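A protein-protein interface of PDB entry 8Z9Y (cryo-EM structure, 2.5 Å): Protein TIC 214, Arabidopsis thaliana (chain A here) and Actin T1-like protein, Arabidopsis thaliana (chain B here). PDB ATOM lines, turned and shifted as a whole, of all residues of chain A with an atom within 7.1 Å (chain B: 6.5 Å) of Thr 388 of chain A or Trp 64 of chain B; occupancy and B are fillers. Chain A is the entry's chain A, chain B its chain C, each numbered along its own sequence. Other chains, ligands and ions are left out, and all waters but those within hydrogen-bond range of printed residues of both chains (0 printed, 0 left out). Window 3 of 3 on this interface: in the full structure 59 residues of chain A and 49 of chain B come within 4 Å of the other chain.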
ATOM      1  N   PHE A 386      -0.732  22.682   7.375  1.00  0.00           N
ATOM      2  CA  PHE A 386      -0.204  21.326   7.403  1.00  0.00           C
ATOM      3  C   PHE A 386       1.218  21.305   7.948  1.00  0.00           C
ATOM      4  O   PHE A 386       2.029  22.181   7.637  1.00  0.00           O
ATOM      5  CB  PHE A 386      -0.231  20.710   6.004  1.00  0.00           C
ATOM      6  CG  PHE A 386      -1.608  20.360   5.521  1.00  0.00           C
ATOM      7  CD1 PHE A 386      -2.406  21.311   4.913  1.00  0.00           C
ATOM      8  CD2 PHE A 386      -2.101  19.076   5.671  1.00  0.00           C
ATOM      9  CE1 PHE A 386      -3.672  20.990   4.465  1.00  0.00           C
ATOM     10  CE2 PHE A 386      -3.366  18.750   5.225  1.00  0.00           C
ATOM     11  CZ  PHE A 386      -4.152  19.707   4.622  1.00  0.00           C
ATOM     12  N   TYR A 387       1.512  20.292   8.760  1.00  0.00           N
ATOM     13  CA  TYR A 387       2.850  20.084   9.293  1.00  0.00           C
ATOM     14  C   TYR A 387       2.974  18.637   9.744  1.00  0.00           C
ATOM     15  O   TYR A 387       1.976  17.973  10.033  1.00  0.00           O
ATOM     16  CB  TYR A 387       3.154  21.036  10.453  1.00  0.00           C
ATOM     17  CG  TYR A 387       4.626  21.173  10.769  1.00  0.00           C
ATOM     18  CD1 TYR A 387       5.492  21.795   9.883  1.00  0.00           C
ATOM     19  CD2 TYR A 387       5.147  20.678  11.957  1.00  0.00           C
ATOM     20  CE1 TYR A 387       6.837  21.920  10.170  1.00  0.00           C
ATOM     21  CE2 TYR A 387       6.489  20.799  12.253  1.00  0.00           C
ATOM     22  CZ  TYR A 387       7.329  21.421  11.356  1.00  0.00           C
ATOM     23  OH  TYR A 387       8.668  21.543  11.647  1.00  0.00           O
ATOM     24  N   THR A 388       4.214  18.161   9.804  1.00  0.00           N
ATOM     25  CA  THR A 388       4.512  16.803  10.239  1.00  0.00           C
ATOM     26  C   THR A 388       5.000  16.840  11.681  1.00  0.00           C
ATOM     27  O   THR A 388       6.038  17.445  11.974  1.00  0.00           O
ATOM     28  CB  THR A 388       5.563  16.153   9.339  1.00  0.00           C
ATOM     29  OG1 THR A 388       6.872  16.507   9.800  1.00  0.00           O
ATOM     30  CG2 THR A 388       5.396  16.620   7.904  1.00  0.00           C
ATOM     31  N   CYS A 389       4.256  16.194  12.575  1.00  0.00           N
ATOM     32  CA  CYS A 389       4.592  16.171  13.990  1.00  0.00           C
ATOM     33  C   CYS A 389       4.415  14.758  14.527  1.00  0.00           C
ATOM     34  O   CYS A 389       3.663  13.952  13.977  1.00  0.00           O
ATOM     35  CB  CYS A 389       3.730  17.156  14.791  1.00  0.00           C
ATOM     36  SG  CYS A 389       4.382  17.564  16.426  1.00  0.00           S
ATOM     37  N   GLN A 390       5.123  14.468  15.615  1.00  0.00           N
ATOM     38  CA  GLN A 390       5.001  13.178  16.283  1.00  0.00           C
ATOM     39  C   GLN A 390       3.706  13.151  17.084  1.00  0.00           C
ATOM     40  O   GLN A 390       3.480  14.017  17.935  1.00  0.00           O
ATOM     41  CB  GLN A 390       6.201  12.932  17.194  1.00  0.00           C
ATOM     42  CG  GLN A 390       7.542  13.283  16.574  1.00  0.00           C
ATOM     43  CD  GLN A 390       8.028  12.231  15.601  1.00  0.00           C
ATOM     44  OE1 GLN A 390       8.198  12.498  14.411  1.00  0.00           O
ATOM     45  NE2 GLN A 390       8.258  11.023  16.102  1.00  0.00           N
ATOM     46  N   GLU A 395       5.416   9.278  13.276  1.00  0.00           N
ATOM     47  CA  GLU A 395       5.295  10.483  12.469  1.00  0.00           C
ATOM     48  C   GLU A 395       3.896  10.579  11.877  1.00  0.00           C
ATOM     49  O   GLU A 395       3.412   9.635  11.245  1.00  0.00           O
ATOM     50  CB  GLU A 395       6.333  10.495  11.349  1.00  0.00           C
ATOM     51  CG  GLU A 395       6.460  11.846  10.666  1.00  0.00           C
ATOM     52  CD  GLU A 395       7.729  11.980   9.856  1.00  0.00           C
ATOM     53  OE1 GLU A 395       8.071  11.024   9.129  1.00  0.00           O
ATOM     54  OE2 GLU A 395       8.385  13.038   9.944  1.00  0.00           O
ATOM     55  N   ARG A 396       3.248  11.723  12.082  1.00  0.00           N
ATOM     56  CA  ARG A 396       1.924  11.979  11.538  1.00  0.00           C
ATOM     57  C   ARG A 396       1.877  13.409  11.022  1.00  0.00           C
ATOM     58  O   ARG A 396       2.739  14.234  11.333  1.00  0.00           O
ATOM     59  CB  ARG A 396       0.827  11.745  12.583  1.00  0.00           C
ATOM     60  CG  ARG A 396       0.710  10.305  13.050  1.00  0.00           C
ATOM     61  CD  ARG A 396       0.027   9.442  12.006  1.00  0.00           C
ATOM     62  NE  ARG A 396      -0.308   8.121  12.523  1.00  0.00           N
ATOM     63  CZ  ARG A 396       0.462   7.051  12.398  1.00  0.00           C
ATOM     64  NH1 ARG A 396       1.631   7.108  11.781  1.00  0.00           N
ATOM     65  NH2 ARG A 396       0.051   5.892  12.905  1.00  0.00           N
ATOM     66  N   ILE A 397       0.855  13.701  10.223  1.00  0.00           N
ATOM     67  CA  ILE A 397       0.659  15.023   9.639  1.00  0.00           C
ATOM     68  C   ILE A 397      -0.471  15.717  10.384  1.00  0.00           C
ATOM     69  O   ILE A 397      -1.572  15.166  10.511  1.00  0.00           O
ATOM     70  CB  ILE A 397       0.363  14.941   8.132  1.00  0.00           C
ATOM     71  CG1 ILE A 397      -0.585  13.781   7.830  1.00  0.00           C
ATOM     72  CG2 ILE A 397       1.652  14.792   7.344  1.00  0.00           C
ATOM     73  CD1 ILE A 397      -0.878  13.608   6.358  1.00  0.00           C
ATOM     74  N   SER A 398      -0.196  16.919  10.879  1.00  0.00           N
ATOM     75  CA  SER A 398      -1.179  17.721  11.596  1.00  0.00           C
ATOM     76  C   SER A 398      -1.699  18.817  10.678  1.00  0.00           C
ATOM     77  O   SER A 398      -0.912  19.538  10.057  1.00  0.00           O
ATOM     78  CB  SER A 398      -0.571  18.331  12.858  1.00  0.00           C
ATOM     79  OG  SER A 398      -1.485  19.212  13.485  1.00  0.00           O
ATOM     80  N   TYR A 401      -1.596  22.980  12.579  1.00  0.00           N
ATOM     81  CA  TYR A 401      -0.367  23.425  13.215  1.00  0.00           C
ATOM     82  C   TYR A 401      -0.243  24.948  13.157  1.00  0.00           C
ATOM     83  O   TYR A 401      -0.696  25.580  12.201  1.00  0.00           O
ATOM     84  CB  TYR A 401       0.837  22.783  12.537  1.00  0.00           C
ATOM     85  CG  TYR A 401       2.033  22.595  13.438  1.00  0.00           C
ATOM     86  CD1 TYR A 401       2.108  21.515  14.306  1.00  0.00           C
ATOM     87  CD2 TYR A 401       3.091  23.492  13.415  1.00  0.00           C
ATOM     88  CE1 TYR A 401       3.201  21.339  15.130  1.00  0.00           C
ATOM     89  CE2 TYR A 401       4.187  23.324  14.235  1.00  0.00           C
ATOM     90  CZ  TYR A 401       4.236  22.246  15.090  1.00  0.00           C
ATOM     91  OH  TYR A 401       5.327  22.073  15.909  1.00  0.00           O
ATOM     92  N   ASP A 427       7.575   6.101  11.071  1.00  0.00           N
ATOM     93  CA  ASP A 427       6.214   5.579  11.141  1.00  0.00           C
ATOM     94  C   ASP A 427       6.030   4.586  12.282  1.00  0.00           C
ATOM     95  O   ASP A 427       4.907   4.426  12.771  1.00  0.00           O
ATOM     96  CB  ASP A 427       5.831   4.926   9.812  1.00  0.00           C
ATOM     97  CG  ASP A 427       6.414   3.535   9.654  1.00  0.00           C
ATOM     98  OD1 ASP A 427       5.751   2.560  10.064  1.00  0.00           O
ATOM     99  OD2 ASP A 427       7.538   3.419   9.122  1.00  0.00           O
ATOM    100  N   PHE B  59      -4.823  14.933  -1.208  1.00  0.00           N
ATOM    101  CA  PHE B  59      -3.709  15.283  -2.084  1.00  0.00           C
ATOM    102  C   PHE B  59      -2.407  15.379  -1.297  1.00  0.00           C
ATOM    103  O   PHE B  59      -1.385  14.784  -1.676  1.00  0.00           O
ATOM    104  CB  PHE B  59      -4.028  16.609  -2.779  1.00  0.00           C
ATOM    105  CG  PHE B  59      -2.978  17.075  -3.744  1.00  0.00           C
ATOM    106  CD1 PHE B  59      -2.959  16.611  -5.046  1.00  0.00           C
ATOM    107  CD2 PHE B  59      -2.029  18.005  -3.357  1.00  0.00           C
ATOM    108  CE1 PHE B  59      -2.006  17.052  -5.939  1.00  0.00           C
ATOM    109  CE2 PHE B  59      -1.070  18.447  -4.245  1.00  0.00           C
ATOM    110  CZ  PHE B  59      -1.060  17.970  -5.538  1.00  0.00           C
ATOM    111  N   GLU B  60      -2.434  16.117  -0.185  1.00  0.00           N
ATOM    112  CA  GLU B  60      -1.235  16.289   0.625  1.00  0.00           C
ATOM    113  C   GLU B  60      -0.768  14.964   1.208  1.00  0.00           C
ATOM    114  O   GLU B  60       0.434  14.693   1.244  1.00  0.00           O
ATOM    115  CB  GLU B  60      -1.488  17.307   1.736  1.00  0.00           C
ATOM    116  CG  GLU B  60      -1.794  18.713   1.241  1.00  0.00           C
ATOM    117  CD  GLU B  60      -0.638  19.342   0.486  1.00  0.00           C
ATOM    118  OE1 GLU B  60       0.517  18.906   0.677  1.00  0.00           O
ATOM    119  OE2 GLU B  60      -0.885  20.278  -0.303  1.00  0.00           O
ATOM    120  N   GLN B  61      -1.699  14.126   1.667  1.00  0.00           N
ATOM    121  CA  GLN B  61      -1.321  12.839   2.238  1.00  0.00           C
ATOM    122  C   GLN B  61      -0.642  11.957   1.201  1.00  0.00           C
ATOM    123  O   GLN B  61       0.410  11.362   1.467  1.00  0.00           O
ATOM    124  CB  GLN B  61      -2.552  12.140   2.814  1.00  0.00           C
ATOM    125  CG  GLN B  61      -2.232  11.062   3.832  1.00  0.00           C
ATOM    126  CD  GLN B  61      -2.889   9.737   3.504  1.00  0.00           C
ATOM    127  OE1 GLN B  61      -3.339   9.517   2.380  1.00  0.00           O
ATOM    128  NE2 GLN B  61      -2.948   8.846   4.484  1.00  0.00           N
ATOM    129  N   TYR B  62      -1.227  11.866   0.004  1.00  0.00           N
ATOM    130  CA  TYR B  62      -0.638  11.022  -1.029  1.00  0.00           C
ATOM    131  C   TYR B  62       0.751  11.512  -1.412  1.00  0.00           C
ATOM    132  O   TYR B  62       1.701  10.721  -1.490  1.00  0.00           O
ATOM    133  CB  TYR B  62      -1.538  10.973  -2.262  1.00  0.00           C
ATOM    134  CG  TYR B  62      -0.794  10.537  -3.500  1.00  0.00           C
ATOM    135  CD1 TYR B  62      -0.315   9.241  -3.622  1.00  0.00           C
ATOM    136  CD2 TYR B  62      -0.552  11.424  -4.539  1.00  0.00           C
ATOM    137  CE1 TYR B  62       0.375   8.838  -4.745  1.00  0.00           C
ATOM    138  CE2 TYR B  62       0.135  11.031  -5.668  1.00  0.00           C
ATOM    139  CZ  TYR B  62       0.599   9.738  -5.764  1.00  0.00           C
ATOM    140  OH  TYR B  62       1.283   9.337  -6.888  1.00  0.00           O
ATOM    141  N   HIS B  63       0.897  12.818  -1.649  1.00  0.00           N
ATOM    142  CA  HIS B  63       2.199  13.313  -2.080  1.00  0.00           C
ATOM    143  C   HIS B  63       3.228  13.256  -0.958  1.00  0.00           C
ATOM    144  O   HIS B  63       4.408  13.003  -1.219  1.00  0.00           O
ATOM    145  CB  HIS B  63       2.066  14.727  -2.637  1.00  0.00           C
ATOM    146  CG  HIS B  63       1.561  14.762  -4.044  1.00  0.00           C
ATOM    147  ND1 HIS B  63       2.283  14.259  -5.104  1.00  0.00           N
ATOM    148  CD2 HIS B  63       0.394  15.209  -4.561  1.00  0.00           C
ATOM    149  CE1 HIS B  63       1.590  14.412  -6.218  1.00  0.00           C
ATOM    150  NE2 HIS B  63       0.440  14.986  -5.916  1.00  0.00           N
ATOM    151  N   TRP B  64       2.804  13.462   0.290  1.00  0.00           N
ATOM    152  CA  TRP B  64       3.705  13.330   1.426  1.00  0.00           C
ATOM    153  C   TRP B  64       4.205  11.900   1.569  1.00  0.00           C
ATOM    154  O   TRP B  64       5.400  11.672   1.797  1.00  0.00           O
ATOM    155  CB  TRP B  64       2.981  13.791   2.691  1.00  0.00           C
ATOM    156  CG  TRP B  64       3.730  13.611   3.967  1.00  0.00           C
ATOM    157  CD1 TRP B  64       4.726  14.403   4.453  1.00  0.00           C
ATOM    158  CD2 TRP B  64       3.516  12.588   4.945  1.00  0.00           C
ATOM    159  NE1 TRP B  64       5.157  13.930   5.668  1.00  0.00           N
ATOM    160  CE2 TRP B  64       4.429  12.816   5.993  1.00  0.00           C
ATOM    161  CE3 TRP B  64       2.646  11.498   5.035  1.00  0.00           C
ATOM    162  CZ2 TRP B  64       4.498  11.993   7.113  1.00  0.00           C
ATOM    163  CZ3 TRP B  64       2.716  10.683   6.149  1.00  0.00           C
ATOM    164  CH2 TRP B  64       3.635  10.934   7.172  1.00  0.00           C
ATOM    165  N   LYS B  65       3.307  10.920   1.433  1.00  0.00           N
ATOM    166  CA  LYS B  65       3.731   9.525   1.489  1.00  0.00           C
ATOM    167  C   LYS B  65       4.680   9.196   0.345  1.00  0.00           C
ATOM    168  O   LYS B  65       5.703   8.531   0.549  1.00  0.00           O
ATOM    169  CB  LYS B  65       2.513   8.603   1.457  1.00  0.00           C
ATOM    170  CG  LYS B  65       2.189   7.959   2.792  1.00  0.00           C
ATOM    171  CD  LYS B  65       0.714   7.619   2.895  1.00  0.00           C
ATOM    172  CE  LYS B  65       0.390   6.964   4.226  1.00  0.00           C
ATOM    173  NZ  LYS B  65       0.855   7.786   5.376  1.00  0.00           N
ATOM    174  N   LYS B  66       4.367   9.669  -0.864  1.00  0.00           N
ATOM    175  CA  LYS B  66       5.236   9.405  -2.007  1.00  0.00           C
ATOM    176  C   LYS B  66       6.617  10.012  -1.802  1.00  0.00           C
ATOM    177  O   LYS B  66       7.632   9.392  -2.140  1.00  0.00           O
ATOM    178  CB  LYS B  66       4.597   9.944  -3.286  1.00  0.00           C
ATOM    179  CG  LYS B  66       5.337   9.564  -4.556  1.00  0.00           C
ATOM    180  CD  LYS B  66       5.045  10.544  -5.682  1.00  0.00           C
ATOM    181  CE  LYS B  66       5.326  11.976  -5.256  1.00  0.00           C
ATOM    182  NZ  LYS B  66       4.802  12.965  -6.239  1.00  0.00           N
ATOM    183  N   ALA B  67       6.678  11.226  -1.251  1.00  0.00           N
ATOM    184  CA  ALA B  67       7.963  11.873  -1.020  1.00  0.00           C
ATOM    185  C   ALA B  67       8.765  11.148   0.052  1.00  0.00           C
ATOM    186  O   ALA B  67       9.951  10.855  -0.140  1.00  0.00           O
ATOM    187  CB  ALA B  67       7.752  13.338  -0.638  1.00  0.00           C
ATOM    188  N   ARG B  68       8.137  10.846   1.191  1.00  0.00           N
ATOM    189  CA  ARG B  68       8.865  10.181   2.267  1.00  0.00           C
ATOM    190  C   ARG B  68       9.176   8.724   1.967  1.00  0.00           C
ATOM    191  O   ARG B  68       9.968   8.121   2.699  1.00  0.00           O
ATOM    192  CB  ARG B  68       8.093  10.276   3.582  1.00  0.00           C
ATOM    193  CG  ARG B  68       7.727  11.686   3.986  1.00  0.00           C
ATOM    194  CD  ARG B  68       7.623  11.789   5.495  1.00  0.00           C
ATOM    195  NE  ARG B  68       8.833  11.308   6.152  1.00  0.00           N
ATOM    196  CZ  ARG B  68       9.990  11.956   6.166  1.00  0.00           C
ATOM    197  NH1 ARG B  68      10.128  13.138   5.588  1.00  0.00           N
ATOM    198  NH2 ARG B  68      11.034  11.405   6.778  1.00  0.00           N
ATOM    199  N   ALA B  69       8.571   8.139   0.931  1.00  0.00           N
ATOM    200  CA  ALA B  69       8.921   6.771   0.568  1.00  0.00           C
ATOM    201  C   ALA B  69      10.389   6.658   0.178  1.00  0.00           C
ATOM    202  O   ALA B  69      11.078   5.720   0.598  1.00  0.00           O
ATOM    203  CB  ALA B  69       8.026   6.287  -0.572  1.00  0.00           C
ATOM    204  N   TYR B  74       9.060  16.839   2.283  1.00  0.00           N
ATOM    205  CA  TYR B  74       7.947  17.297   1.464  1.00  0.00           C
ATOM    206  C   TYR B  74       7.431  18.622   2.003  1.00  0.00           C
ATOM    207  O   TYR B  74       7.204  18.759   3.209  1.00  0.00           O
ATOM    208  CB  TYR B  74       6.823  16.258   1.440  1.00  0.00           C
ATOM    209  CG  TYR B  74       5.619  16.686   0.641  1.00  0.00           C
ATOM    210  CD1 TYR B  74       5.653  16.699  -0.745  1.00  0.00           C
ATOM    211  CD2 TYR B  74       4.451  17.086   1.272  1.00  0.00           C
ATOM    212  CE1 TYR B  74       4.556  17.095  -1.481  1.00  0.00           C
ATOM    213  CE2 TYR B  74       3.350  17.484   0.546  1.00  0.00           C
ATOM    214  CZ  TYR B  74       3.407  17.486  -0.831  1.00  0.00           C
ATOM    215  OH  TYR B  74       2.310  17.882  -1.559  1.00  0.00           O
ATOM    216  N   PHE B  76       4.309  21.363   1.841  1.00  0.00           N
ATOM    217  CA  PHE B  76       2.881  21.292   1.568  1.00  0.00           C
ATOM    218  C   PHE B  76       2.447  22.455   0.686  1.00  0.00           C
ATOM    219  O   PHE B  76       2.797  23.610   0.948  1.00  0.00           O
ATOM    220  CB  PHE B  76       2.092  21.286   2.875  1.00  0.00           C
ATOM    221  CG  PHE B  76       2.388  20.103   3.752  1.00  0.00           C
ATOM    222  CD1 PHE B  76       1.660  18.934   3.631  1.00  0.00           C
ATOM    223  CD2 PHE B  76       3.397  20.163   4.697  1.00  0.00           C
ATOM    224  CE1 PHE B  76       1.932  17.845   4.435  1.00  0.00           C
ATOM    225  CE2 PHE B  76       3.673  19.078   5.505  1.00  0.00           C
ATOM    226  CZ  PHE B  76       2.940  17.918   5.374  1.00  0.00           C
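The side-chain carboxylate (OE1) of Glu 395 of chain A lies within salt-bridge range of the guanidinium group (NE) of Arg 68 of chain B.
Phe 76 of chain B touches Phe 386 of chain A.
Thr 388 of chain A touches Trp 64 of chain B (CG2 to NE1, 3.5 Å).
Thr 388 of chain A touches Phe 76 of chain B (CG2 to CZ, 3.8 Å).
Ile 397 of chain A touches Gln 61 of chain B (CD1 to CG, 3.8 Å).
Trp 64 of chain B touches Ile 397 of chain A.
Phe 76 of chain B touches Ile 397 of chain A (CZ to CG2, 3.9 Å).
Thr 388 of chain A touches just these residues of chain B: Trp 64 and Phe 76.
Of chain A, only Thr 388 (3.5 Å) and Ile 397 (3.7 Å) come within 4 Å of Trp 64 of chain B.
Of the printed residues of chain B, Glu 395 of chain A touches Arg 68 (3.1 Å).
Of the printed residues of chain A, Gln 61 of chain B touches Ile 397.
Of the printed residues of chain A, Arg 68 of chain B touches Glu 395 (3.1 Å).
Printed residues of chain A within 4 Å of Phe 76 of chain B: Phe 386, Thr 388 and Ile 397.
Printed residues of chain B within 4 Å of Phe 386 of chain A: Phe 76.
Cys 389 of chain A touches none of the printed residues of chain B.
Tyr 387 of chain A touches none of the printed residues of chain B.
The nearest residue of chain B that does not touch Thr 388 of chain A is Tyr 74 of chain B (5.5 Å).
The nearest residue of chain A that does not touch Trp 64 of chain B is Glu 395 of chain A (4.1 Å).
Printed residues of chain A that touch a printed residue of chain B: Phe 386, Thr 388, Glu 395 and Ile 397.
Of the 13 printed residues of chain B, 4 touch a printed residue of chain A.
Printed residues of chain B that touch a printed residue of chain A: Gln 61, Trp 64, Arg 68 and Phe 76.
Hydrophobic or aromatic side chains of chain B that line the printed part of chain A: Trp 64 and Phe 76.
Among the printed residues, 7 pairs touch across the chains.
Among the printed residues, Asp or Glu carboxylates within 4 Å of a Lys or Arg side-chain nitrogen of the other chain: Glu 395 of chain A with Arg 68 of chain B (3.1 Å).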
